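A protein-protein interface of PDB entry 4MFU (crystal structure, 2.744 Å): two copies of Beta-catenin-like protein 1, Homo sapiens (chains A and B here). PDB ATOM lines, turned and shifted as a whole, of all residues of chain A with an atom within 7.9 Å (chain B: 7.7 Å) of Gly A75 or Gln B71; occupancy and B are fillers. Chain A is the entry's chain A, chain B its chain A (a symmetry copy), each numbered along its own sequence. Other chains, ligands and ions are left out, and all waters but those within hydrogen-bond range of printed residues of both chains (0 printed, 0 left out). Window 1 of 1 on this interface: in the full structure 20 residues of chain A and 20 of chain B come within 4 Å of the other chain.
The backbone carbonyl oxygen (O) of Val B65 lies within hydrogen-bond range of the side-chain amide nitrogen (ND2) of Asn B68 (3.5 Å). The backbone carbonyl oxygen (O) of Glu B66 is in hydrogen-bond range of the side-chain amide nitrogen (ND2) of Asn B68 (3.2 Å). The side-chain amide oxygen (OD1) of Asn B68 lies close to the side-chain amide nitrogen (NE2) of Gln B71, at 3.0 Å. The backbone carbonyl oxygen (O) of Asn B68 is in hydrogen-bond range of the side-chain hydroxyl (OG) of Ser B72, at 3.3 Å.
Asn B68 touches Gln A24. OE1 of Gln A71 touches CA of Gly B75, at 3.8 Å. OE1 of Gln B71 touches CA of Gly A75 (3.8 Å).
Gly A75 touches just one residue of chain B: Gln B71. Gln B71 touches just one residue of chain A: Gly A75. No residue of chain A comes within 4 Å of Val B70. Of the printed residues of chain A, Asn B68 touches Gln A24. Of the printed residues of chain B, Gln A24 touches Asn B68. Of the printed residues of chain A, Gly B75 touches Gln A71 (3.8 Å). The nearest residue of chain B that does not touch Gly A75 is Asn B68 (5.8 Å). The nearest residue of chain A that does not touch Gln B71 is Gly A78 (4.8 Å).
Of the 20 printed residues of chain B, 3 touch a printed residue of chain A. Printed residues of chain B that touch a printed residue of chain A: Asn B68, Gln B71 and Gly B75. Of the 21 printed residues of chain A, 3 touch a printed residue of chain B. Along chain A the printed residues that touch a printed residue of chain B span positions 24 to 75. Among the printed residues, 3 pairs touch across the chains. Among the printed residues, no Asp or Glu carboxylate lies within 4 Å of a Lys or Arg side-chain nitrogen of the other chain.
Gln A71 touches Gly B75, and with the chains exchanged Gly A75 touches Gln B71. Positions printed for both chains: 16, 69, 70, 71, 72, 73, 74, 75, 76, 77, 88, 118 and 123.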
ATOM      1  N   PHE A  16      12.282 -17.667   2.451  1.00  0.00           N
ATOM      2  CA  PHE A  16      11.456 -16.531   2.076  1.00  0.00           C
ATOM      3  C   PHE A  16      12.035 -15.210   2.610  1.00  0.00           C
ATOM      4  O   PHE A  16      12.184 -14.220   1.866  1.00  0.00           O
ATOM      5  CB  PHE A  16      10.026 -16.781   2.576  1.00  0.00           C
ATOM      6  CG  PHE A  16       9.140 -15.558   2.564  1.00  0.00           C
ATOM      7  CD1 PHE A  16       8.910 -14.855   1.387  1.00  0.00           C
ATOM      8  CD2 PHE A  16       8.528 -15.120   3.734  1.00  0.00           C
ATOM      9  CE1 PHE A  16       8.098 -13.740   1.381  1.00  0.00           C
ATOM     10  CE2 PHE A  16       7.725 -13.997   3.735  1.00  0.00           C
ATOM     11  CZ  PHE A  16       7.503 -13.315   2.551  1.00  0.00           C
ATOM     12  N   SER A  20      13.587 -12.047   0.638  1.00  0.00           N
ATOM     13  CA  SER A  20      13.108 -10.681   0.723  1.00  0.00           C
ATOM     14  C   SER A  20      14.241  -9.666   0.953  1.00  0.00           C
ATOM     15  O   SER A  20      14.320  -8.597   0.297  1.00  0.00           O
ATOM     16  CB  SER A  20      12.101 -10.593   1.862  1.00  0.00           C
ATOM     17  OG  SER A  20      11.538  -9.295   1.926  1.00  0.00           O
ATOM     18  N   GLN A  24      15.704  -6.686  -0.967  1.00  0.00           N
ATOM     19  CA  GLN A  24      15.759  -5.426  -0.324  1.00  0.00           C
ATOM     20  C   GLN A  24      17.076  -4.767  -0.660  1.00  0.00           C
ATOM     21  O   GLN A  24      17.075  -3.673  -1.222  1.00  0.00           O
ATOM     22  CB  GLN A  24      15.568  -5.533   1.184  1.00  0.00           C
ATOM     23  CG  GLN A  24      15.201  -4.200   1.815  1.00  0.00           C
ATOM     24  CD  GLN A  24      14.112  -3.473   1.043  1.00  0.00           C
ATOM     25  OE1 GLN A  24      12.937  -3.597   1.363  1.00  0.00           O
ATOM     26  NE2 GLN A  24      14.497  -2.732   0.001  1.00  0.00           N
ATOM     27  N   ALA A  69       6.495 -14.344   9.088  1.00  0.00           N
ATOM     28  CA  ALA A  69       6.192 -14.475   7.674  1.00  0.00           C
ATOM     29  C   ALA A  69       5.105 -13.479   7.345  1.00  0.00           C
ATOM     30  O   ALA A  69       5.194 -12.690   6.382  1.00  0.00           O
ATOM     31  CB  ALA A  69       5.711 -15.890   7.374  1.00  0.00           C
ATOM     32  N   VAL A  70       4.070 -13.551   8.172  1.00  0.00           N
ATOM     33  CA  VAL A  70       2.908 -12.698   8.053  1.00  0.00           C
ATOM     34  C   VAL A  70       3.343 -11.261   7.750  1.00  0.00           C
ATOM     35  O   VAL A  70       3.038 -10.721   6.665  1.00  0.00           O
ATOM     36  CB  VAL A  70       2.032 -12.809   9.337  1.00  0.00           C
ATOM     37  CG1 VAL A  70       2.827 -12.486  10.609  1.00  0.00           C
ATOM     38  CG2 VAL A  70       0.786 -11.946   9.229  1.00  0.00           C
ATOM     39  N   GLN A  71       4.137 -10.703   8.669  1.00  0.00           N
ATOM     40  CA  GLN A  71       4.431  -9.289   8.681  1.00  0.00           C
ATOM     41  C   GLN A  71       5.089  -8.951   7.380  1.00  0.00           C
ATOM     42  O   GLN A  71       4.555  -8.161   6.600  1.00  0.00           O
ATOM     43  CB  GLN A  71       5.326  -8.909   9.863  1.00  0.00           C
ATOM     44  CG  GLN A  71       4.683  -9.108  11.243  1.00  0.00           C
ATOM     45  CD  GLN A  71       5.419  -8.377  12.375  1.00  0.00           C
ATOM     46  OE1 GLN A  71       6.163  -7.409  12.140  1.00  0.00           O
ATOM     47  NE2 GLN A  71       5.212  -8.843  13.620  1.00  0.00           N
ATOM     48  N   SER A  72       6.224  -9.593   7.120  1.00  0.00           N
ATOM     49  CA  SER A  72       6.953  -9.386   5.877  1.00  0.00           C
ATOM     50  C   SER A  72       5.952  -9.440   4.747  1.00  0.00           C
ATOM     51  O   SER A  72       5.835  -8.498   3.972  1.00  0.00           O
ATOM     52  CB  SER A  72       8.032 -10.454   5.700  1.00  0.00           C
ATOM     53  OG  SER A  72       9.032 -10.355   6.714  1.00  0.00           O
ATOM     54  N   LEU A  73       5.174 -10.518   4.710  1.00  0.00           N
ATOM     55  CA  LEU A  73       4.154 -10.693   3.681  1.00  0.00           C
ATOM     56  C   LEU A  73       3.334  -9.479   3.496  1.00  0.00           C
ATOM     57  O   LEU A  73       3.280  -8.923   2.383  1.00  0.00           O
ATOM     58  CB  LEU A  73       3.217 -11.836   4.023  1.00  0.00           C
ATOM     59  CG  LEU A  73       3.733 -13.118   3.399  1.00  0.00           C
ATOM     60  CD1 LEU A  73       3.199 -14.338   4.114  1.00  0.00           C
ATOM     61  CD2 LEU A  73       3.369 -13.149   1.927  1.00  0.00           C
ATOM     62  N   LEU A  74       2.687  -9.079   4.592  1.00  0.00           N
ATOM     63  CA  LEU A  74       1.927  -7.835   4.600  1.00  0.00           C
ATOM     64  C   LEU A  74       2.773  -6.695   4.067  1.00  0.00           C
ATOM     65  O   LEU A  74       2.334  -5.955   3.194  1.00  0.00           O
ATOM     66  CB  LEU A  74       1.409  -7.496   5.989  1.00  0.00           C
ATOM     67  CG  LEU A  74       0.293  -8.390   6.521  1.00  0.00           C
ATOM     68  CD1 LEU A  74      -0.379  -7.778   7.745  1.00  0.00           C
ATOM     69  CD2 LEU A  74      -0.744  -8.664   5.449  1.00  0.00           C
ATOM     70  N   GLY A  75       3.998  -6.595   4.569  1.00  0.00           N
ATOM     71  CA  GLY A  75       4.945  -5.603   4.089  1.00  0.00           C
ATOM     72  C   GLY A  75       4.922  -5.516   2.584  1.00  0.00           C
ATOM     73  O   GLY A  75       4.752  -4.442   2.014  1.00  0.00           O
ATOM     74  N   LEU A  76       5.032  -6.666   1.934  1.00  0.00           N
ATOM     75  CA  LEU A  76       5.201  -6.708   0.483  1.00  0.00           C
ATOM     76  C   LEU A  76       3.961  -6.321  -0.308  1.00  0.00           C
ATOM     77  O   LEU A  76       4.010  -6.164  -1.543  1.00  0.00           O
ATOM     78  CB  LEU A  76       5.643  -8.094   0.069  1.00  0.00           C
ATOM     79  CG  LEU A  76       7.111  -8.377   0.327  1.00  0.00           C
ATOM     80  CD1 LEU A  76       7.530  -8.041   1.743  1.00  0.00           C
ATOM     81  CD2 LEU A  76       7.388  -9.846   0.049  1.00  0.00           C
ATOM     82  N   LEU A  77       2.846  -6.163   0.393  1.00  0.00           N
ATOM     83  CA  LEU A  77       1.626  -5.694  -0.261  1.00  0.00           C
ATOM     84  C   LEU A  77       1.885  -4.314  -0.834  1.00  0.00           C
ATOM     85  O   LEU A  77       1.246  -3.898  -1.810  1.00  0.00           O
ATOM     86  CB  LEU A  77       0.441  -5.673   0.700  1.00  0.00           C
ATOM     87  CG  LEU A  77      -0.244  -7.027   0.892  1.00  0.00           C
ATOM     88  CD1 LEU A  77       0.769  -8.111   1.178  1.00  0.00           C
ATOM     89  CD2 LEU A  77      -1.191  -6.962   2.055  1.00  0.00           C
ATOM     90  N   GLY A  78       2.867  -3.632  -0.264  1.00  0.00           N
ATOM     91  CA  GLY A  78       3.369  -2.422  -0.869  1.00  0.00           C
ATOM     92  C   GLY A  78       4.718  -2.727  -1.471  1.00  0.00           C
ATOM     93  O   GLY A  78       5.684  -2.993  -0.768  1.00  0.00           O
ATOM     94  N   HIS A  79       4.774  -2.691  -2.790  1.00  0.00           N
ATOM     95  CA  HIS A  79       5.998  -2.927  -3.520  1.00  0.00           C
ATOM     96  C   HIS A  79       5.865  -2.108  -4.770  1.00  0.00           C
ATOM     97  O   HIS A  79       4.756  -1.900  -5.255  1.00  0.00           O
ATOM     98  CB  HIS A  79       6.120  -4.403  -3.870  1.00  0.00           C
ATOM     99  CG  HIS A  79       7.478  -4.804  -4.349  1.00  0.00           C
ATOM    100  ND1 HIS A  79       7.861  -4.701  -5.667  1.00  0.00           N
ATOM    101  CD2 HIS A  79       8.538  -5.325  -3.690  1.00  0.00           C
ATOM    102  CE1 HIS A  79       9.100  -5.134  -5.798  1.00  0.00           C
ATOM    103  NE2 HIS A  79       9.533  -5.519  -4.613  1.00  0.00           N
ATOM    104  N   VAL A  84       4.470  -8.567  -7.587  1.00  0.00           N
ATOM    105  CA  VAL A  84       4.771  -9.088  -6.254  1.00  0.00           C
ATOM    106  C   VAL A  84       3.585  -8.875  -5.303  1.00  0.00           C
ATOM    107  O   VAL A  84       3.293  -9.710  -4.437  1.00  0.00           O
ATOM    108  CB  VAL A  84       6.083  -8.478  -5.678  1.00  0.00           C
ATOM    109  CG1 VAL A  84       6.170  -7.000  -5.983  1.00  0.00           C
ATOM    110  CG2 VAL A  84       6.220  -8.703  -4.168  1.00  0.00           C
ATOM    111  N   SER A  85       2.890  -7.762  -5.467  1.00  0.00           N
ATOM    112  CA  SER A  85       1.747  -7.467  -4.617  1.00  0.00           C
ATOM    113  C   SER A  85       0.711  -8.530  -4.899  1.00  0.00           C
ATOM    114  O   SER A  85       0.462  -9.403  -4.051  1.00  0.00           O
ATOM    115  CB  SER A  85       1.244  -6.056  -4.899  1.00  0.00           C
ATOM    116  OG  SER A  85       2.080  -5.128  -4.221  1.00  0.00           O
ATOM    117  N   VAL A  88       1.212 -11.680  -3.439  1.00  0.00           N
ATOM    118  CA  VAL A  88       1.047 -11.846  -2.005  1.00  0.00           C
ATOM    119  C   VAL A  88      -0.427 -11.993  -1.720  1.00  0.00           C
ATOM    120  O   VAL A  88      -0.850 -12.752  -0.836  1.00  0.00           O
ATOM    121  CB  VAL A  88       1.658 -10.691  -1.186  1.00  0.00           C
ATOM    122  CG1 VAL A  88       1.457 -10.963   0.288  1.00  0.00           C
ATOM    123  CG2 VAL A  88       3.153 -10.585  -1.438  1.00  0.00           C
ATOM    124  N   GLY A 118      -2.146  -6.649  11.955  1.00  0.00           N
ATOM    125  CA  GLY A 118      -1.281  -5.989  11.018  1.00  0.00           C
ATOM    126  C   GLY A 118      -2.005  -5.075  10.078  1.00  0.00           C
ATOM    127  O   GLY A 118      -1.418  -4.625   9.083  1.00  0.00           O
ATOM    128  N   LEU A 123      -3.996  -2.240   4.311  1.00  0.00           N
ATOM    129  CA  LEU A 123      -2.947  -2.530   3.354  1.00  0.00           C
ATOM    130  C   LEU A 123      -3.555  -3.053   2.049  1.00  0.00           C
ATOM    131  O   LEU A 123      -3.154  -2.631   0.970  1.00  0.00           O
ATOM    132  CB  LEU A 123      -1.944  -3.517   3.970  1.00  0.00           C
ATOM    133  CG  LEU A 123      -1.432  -3.101   5.369  1.00  0.00           C
ATOM    134  CD1 LEU A 123      -0.694  -4.254   6.025  1.00  0.00           C
ATOM    135  CD2 LEU A 123      -0.578  -1.827   5.348  1.00  0.00           C
ATOM    136  N   GLN A 126      -5.001  -0.246  -0.048  1.00  0.00           N
ATOM    137  CA  GLN A 126      -3.937   0.581  -0.631  1.00  0.00           C
ATOM    138  C   GLN A 126      -3.525  -0.072  -1.931  1.00  0.00           C
ATOM    139  O   GLN A 126      -3.562   0.561  -3.000  1.00  0.00           O
ATOM    140  CB  GLN A 126      -2.715   0.721   0.293  1.00  0.00           C
ATOM    141  CG  GLN A 126      -2.852   1.763   1.398  1.00  0.00           C
ATOM    142  CD  GLN A 126      -1.659   1.788   2.356  1.00  0.00           C
ATOM    143  OE1 GLN A 126      -0.512   1.657   1.936  1.00  0.00           O
ATOM    144  NE2 GLN A 126      -1.931   1.970   3.647  1.00  0.00           N
ATOM    145  N   ASN A 127      -3.152  -1.346  -1.834  1.00  0.00           N
ATOM    146  CA  ASN A 127      -2.859  -2.153  -3.020  1.00  0.00           C
ATOM    147  C   ASN A 127      -4.050  -2.017  -3.976  1.00  0.00           C
ATOM    148  O   ASN A 127      -3.948  -1.497  -5.088  1.00  0.00           O
ATOM    149  CB  ASN A 127      -2.621  -3.621  -2.595  1.00  0.00           C
ATOM    150  CG  ASN A 127      -1.742  -4.425  -3.567  1.00  0.00           C
ATOM    151  OD1 ASN A 127      -1.656  -4.144  -4.769  1.00  0.00           O
ATOM    152  ND2 ASN A 127      -1.118  -5.477  -3.034  1.00  0.00           N
ATOM    153  N   PHE B  16      21.212  -1.396   9.811  1.00  0.00           N
ATOM    154  CA  PHE B  16      20.022  -1.620  10.615  1.00  0.00           C
ATOM    155  C   PHE B  16      19.231  -2.846  10.128  1.00  0.00           C
ATOM    156  O   PHE B  16      18.858  -3.734  10.919  1.00  0.00           O
ATOM    157  CB  PHE B  16      19.174  -0.339  10.601  1.00  0.00           C
ATOM    158  CG  PHE B  16      17.762  -0.523  11.103  1.00  0.00           C
ATOM    159  CD1 PHE B  16      17.516  -1.011  12.381  1.00  0.00           C
ATOM    160  CD2 PHE B  16      16.678  -0.194  10.294  1.00  0.00           C
ATOM    161  CE1 PHE B  16      16.225  -1.174  12.836  1.00  0.00           C
ATOM    162  CE2 PHE B  16      15.384  -0.368  10.741  1.00  0.00           C
ATOM    163  CZ  PHE B  16      15.161  -0.849  12.019  1.00  0.00           C
ATOM    164  N   LEU B  64      14.903   6.947   4.579  1.00  0.00           N
ATOM    165  CA  LEU B  64      14.267   6.048   5.545  1.00  0.00           C
ATOM    166  C   LEU B  64      13.012   5.284   5.102  1.00  0.00           C
ATOM    167  O   LEU B  64      12.684   4.251   5.685  1.00  0.00           O
ATOM    168  CB  LEU B  64      13.868   6.866   6.748  1.00  0.00           C
ATOM    169  CG  LEU B  64      15.011   7.190   7.668  1.00  0.00           C
ATOM    170  CD1 LEU B  64      14.719   8.508   8.340  1.00  0.00           C
ATOM    171  CD2 LEU B  64      15.169   6.073   8.677  1.00  0.00           C
ATOM    172  N   VAL B  65      12.293   5.817   4.122  1.00  0.00           N
ATOM    173  CA  VAL B  65      10.984   5.281   3.761  1.00  0.00           C
ATOM    174  C   VAL B  65      11.041   4.412   2.510  1.00  0.00           C
ATOM    175  O   VAL B  65      10.475   3.311   2.497  1.00  0.00           O
ATOM    176  CB  VAL B  65       9.912   6.390   3.591  1.00  0.00           C
ATOM    177  CG1 VAL B  65      10.345   7.453   2.598  1.00  0.00           C
ATOM    178  CG2 VAL B  65       8.577   5.794   3.153  1.00  0.00           C
ATOM    179  N   GLU B  66      11.713   4.893   1.465  1.00  0.00           N
ATOM    180  CA  GLU B  66      11.852   4.103   0.245  1.00  0.00           C
ATOM    181  C   GLU B  66      12.707   2.894   0.603  1.00  0.00           C
ATOM    182  O   GLU B  66      12.368   1.762   0.262  1.00  0.00           O
ATOM    183  CB  GLU B  66      12.451   4.926  -0.914  1.00  0.00           C
ATOM    184  CG  GLU B  66      12.306   4.295  -2.310  1.00  0.00           C
ATOM    185  CD  GLU B  66      10.854   4.036  -2.754  1.00  0.00           C
ATOM    186  OE1 GLU B  66       9.922   4.700  -2.246  1.00  0.00           O
ATOM    187  OE2 GLU B  66      10.636   3.160  -3.629  1.00  0.00           O
ATOM    188  N   LEU B  67      13.759   3.131   1.374  1.00  0.00           N
ATOM    189  CA  LEU B  67      14.643   2.060   1.810  1.00  0.00           C
ATOM    190  C   LEU B  67      14.044   1.232   2.975  1.00  0.00           C
ATOM    191  O   LEU B  67      14.697   0.351   3.530  1.00  0.00           O
ATOM    192  CB  LEU B  67      16.015   2.633   2.164  1.00  0.00           C
ATOM    193  CG  LEU B  67      16.806   3.199   0.964  1.00  0.00           C
ATOM    194  CD1 LEU B  67      16.132   4.360   0.224  1.00  0.00           C
ATOM    195  CD2 LEU B  67      18.201   3.610   1.414  1.00  0.00           C
ATOM    196  N   ASN B  68      12.796   1.521   3.332  1.00  0.00           N
ATOM    197  CA  ASN B  68      11.989   0.654   4.201  1.00  0.00           C
ATOM    198  C   ASN B  68      12.467   0.510   5.640  1.00  0.00           C
ATOM    199  O   ASN B  68      12.259  -0.528   6.278  1.00  0.00           O
ATOM    200  CB  ASN B  68      11.804  -0.720   3.558  1.00  0.00           C
ATOM    201  CG  ASN B  68      10.475  -0.839   2.852  1.00  0.00           C
ATOM    202  OD1 ASN B  68       9.604  -1.591   3.293  1.00  0.00           O
ATOM    203  ND2 ASN B  68      10.296  -0.077   1.766  1.00  0.00           N
ATOM    204  N   ALA B  69      13.072   1.581   6.142  1.00  0.00           N
ATOM    205  CA  ALA B  69      13.467   1.671   7.537  1.00  0.00           C
ATOM    206  C   ALA B  69      12.207   1.737   8.366  1.00  0.00           C
ATOM    207  O   ALA B  69      12.018   0.993   9.350  1.00  0.00           O
ATOM    208  CB  ALA B  69      14.305   2.924   7.762  1.00  0.00           C
ATOM    209  N   VAL B  70      11.356   2.661   7.942  1.00  0.00           N
ATOM    210  CA  VAL B  70      10.082   2.911   8.579  1.00  0.00           C
ATOM    211  C   VAL B  70       9.406   1.583   8.934  1.00  0.00           C
ATOM    212  O   VAL B  70       9.202   1.273  10.128  1.00  0.00           O
ATOM    213  CB  VAL B  70       9.199   3.818   7.670  1.00  0.00           C
ATOM    214  CG1 VAL B  70       9.008   3.222   6.270  1.00  0.00           C
ATOM    215  CG2 VAL B  70       7.864   4.123   8.328  1.00  0.00           C
ATOM    216  N   GLN B  71       9.165   0.775   7.897  1.00  0.00           N
ATOM    217  CA  GLN B  71       8.314  -0.387   8.004  1.00  0.00           C
ATOM    218  C   GLN B  71       8.907  -1.291   9.038  1.00  0.00           C
ATOM    219  O   GLN B  71       8.282  -1.557  10.066  1.00  0.00           O
ATOM    220  CB  GLN B  71       8.173  -1.109   6.660  1.00  0.00           C
ATOM    221  CG  GLN B  71       7.460  -0.296   5.570  1.00  0.00           C
ATOM    222  CD  GLN B  71       6.987  -1.146   4.382  1.00  0.00           C
ATOM    223  OE1 GLN B  71       6.813  -2.372   4.496  1.00  0.00           O
ATOM    224  NE2 GLN B  71       6.776  -0.491   3.226  1.00  0.00           N
ATOM    225  N   SER B  72      10.141  -1.721   8.793  1.00  0.00           N
ATOM    226  CA  SER B  72      10.853  -2.580   9.729  1.00  0.00           C
ATOM    227  C   SER B  72      10.677  -1.994  11.110  1.00  0.00           C
ATOM    228  O   SER B  72      10.189  -2.662  12.014  1.00  0.00           O
ATOM    229  CB  SER B  72      12.333  -2.670   9.360  1.00  0.00           C
ATOM    230  OG  SER B  72      12.516  -3.304   8.095  1.00  0.00           O
ATOM    231  N   LEU B  73      11.003  -0.712  11.243  1.00  0.00           N
ATOM    232  CA  LEU B  73      10.869  -0.014  12.518  1.00  0.00           C
ATOM    233  C   LEU B  73       9.562  -0.265  13.157  1.00  0.00           C
ATOM    234  O   LEU B  73       9.505  -0.772  14.293  1.00  0.00           O
ATOM    235  CB  LEU B  73      11.017   1.486  12.344  1.00  0.00           C
ATOM    236  CG  LEU B  73      12.467   1.879  12.550  1.00  0.00           C
ATOM    237  CD1 LEU B  73      12.787   3.196  11.880  1.00  0.00           C
ATOM    238  CD2 LEU B  73      12.774   1.935  14.033  1.00  0.00           C
ATOM    239  N   LEU B  74       8.510   0.103  12.422  1.00  0.00           N
ATOM    240  CA  LEU B  74       7.150  -0.183  12.866  1.00  0.00           C
ATOM    241  C   LEU B  74       7.015  -1.643  13.247  1.00  0.00           C
ATOM    242  O   LEU B  74       6.514  -1.958  14.321  1.00  0.00           O
ATOM    243  CB  LEU B  74       6.121   0.179  11.807  1.00  0.00           C
ATOM    244  CG  LEU B  74       5.918   1.670  11.557  1.00  0.00           C
ATOM    245  CD1 LEU B  74       4.654   1.934  10.745  1.00  0.00           C
ATOM    246  CD2 LEU B  74       5.858   2.440  12.862  1.00  0.00           C
ATOM    247  N   GLY B  75       7.506  -2.520  12.380  1.00  0.00           N
ATOM    248  CA  GLY B  75       7.521  -3.947  12.656  1.00  0.00           C
ATOM    249  C   GLY B  75       7.956  -4.220  14.072  1.00  0.00           C
ATOM    250  O   GLY B  75       7.271  -4.908  14.825  1.00  0.00           O
ATOM    251  N   LEU B  76       9.077  -3.627  14.460  1.00  0.00           N
ATOM    252  CA  LEU B  76       9.703  -3.945  15.741  1.00  0.00           C
ATOM    253  C   LEU B  76       8.949  -3.430  16.957  1.00  0.00           C
ATOM    254  O   LEU B  76       9.286  -3.762  18.110  1.00  0.00           O
ATOM    255  CB  LEU B  76      11.112  -3.397  15.761  1.00  0.00           C
ATOM    256  CG  LEU B  76      12.111  -4.230  14.977  1.00  0.00           C
ATOM    257  CD1 LEU B  76      11.635  -4.540  13.573  1.00  0.00           C
ATOM    258  CD2 LEU B  76      13.433  -3.484  14.914  1.00  0.00           C
ATOM    259  N   LEU B  77       7.927  -2.622  16.712  1.00  0.00           N
ATOM    260  CA  LEU B  77       7.078  -2.154  17.807  1.00  0.00           C
ATOM    261  C   LEU B  77       6.431  -3.359  18.463  1.00  0.00           C
ATOM    262  O   LEU B  77       6.078  -3.326  19.651  1.00  0.00           O
ATOM    263  CB  LEU B  77       6.025  -1.163  17.323  1.00  0.00           C
ATOM    264  CG  LEU B  77       6.529   0.273  17.170  1.00  0.00           C
ATOM    265  CD1 LEU B  77       7.823   0.313  16.393  1.00  0.00           C
ATOM    266  CD2 LEU B  77       5.517   1.095  16.425  1.00  0.00           C
ATOM    267  N   VAL B  88      12.246   1.681  19.972  1.00  0.00           N
ATOM    268  CA  VAL B  88      11.778   2.133  18.673  1.00  0.00           C
ATOM    269  C   VAL B  88      10.904   3.343  18.888  1.00  0.00           C
ATOM    270  O   VAL B  88      10.898   4.296  18.096  1.00  0.00           O
ATOM    271  CB  VAL B  88      11.030   1.041  17.883  1.00  0.00           C
ATOM    272  CG1 VAL B  88      10.603   1.596  16.543  1.00  0.00           C
ATOM    273  CG2 VAL B  88      11.936  -0.152  17.624  1.00  0.00           C
ATOM    274  N   ALA B 114       4.469   7.793   5.462  1.00  0.00           N
ATOM    275  CA  ALA B 114       4.790   6.388   5.699  1.00  0.00           C
ATOM    276  C   ALA B 114       4.173   5.863   7.003  1.00  0.00           C
ATOM    277  O   ALA B 114       3.395   4.911   7.001  1.00  0.00           O
ATOM    278  CB  ALA B 114       6.301   6.185   5.710  1.00  0.00           C
ATOM    279  N   LEU B 115       4.496   6.505   8.110  1.00  0.00           N
ATOM    280  CA  LEU B 115       3.965   6.098   9.415  1.00  0.00           C
ATOM    281  C   LEU B 115       2.454   5.889   9.424  1.00  0.00           C
ATOM    282  O   LEU B 115       1.949   4.887   9.921  1.00  0.00           O
ATOM    283  CB  LEU B 115       4.294   7.161  10.455  1.00  0.00           C
ATOM    284  CG  LEU B 115       5.774   7.272  10.776  1.00  0.00           C
ATOM    285  CD1 LEU B 115       6.099   8.628  11.395  1.00  0.00           C
ATOM    286  CD2 LEU B 115       6.182   6.126  11.694  1.00  0.00           C
ATOM    287  N   GLY B 118       1.341   3.103   7.618  1.00  0.00           N
ATOM    288  CA  GLY B 118       1.702   1.888   8.293  1.00  0.00           C
ATOM    289  C   GLY B 118       0.927   1.653   9.553  1.00  0.00           C
ATOM    290  O   GLY B 118       1.293   0.772  10.345  1.00  0.00           O
ATOM    291  N   LEU B 123      -0.354   0.297  16.017  1.00  0.00           N
ATOM    292  CA  LEU B 123       0.813  -0.415  16.502  1.00  0.00           C
ATOM    293  C   LEU B 123       1.271   0.176  17.839  1.00  0.00           C
ATOM    294  O   LEU B 123       1.574  -0.565  18.767  1.00  0.00           O
ATOM    295  CB  LEU B 123       1.919  -0.382  15.437  1.00  0.00           C
ATOM    296  CG  LEU B 123       1.447  -0.817  14.028  1.00  0.00           C
ATOM    297  CD1 LEU B 123       2.501  -0.474  12.991  1.00  0.00           C
ATOM    298  CD2 LEU B 123       1.045  -2.295  13.954  1.00  0.00           C
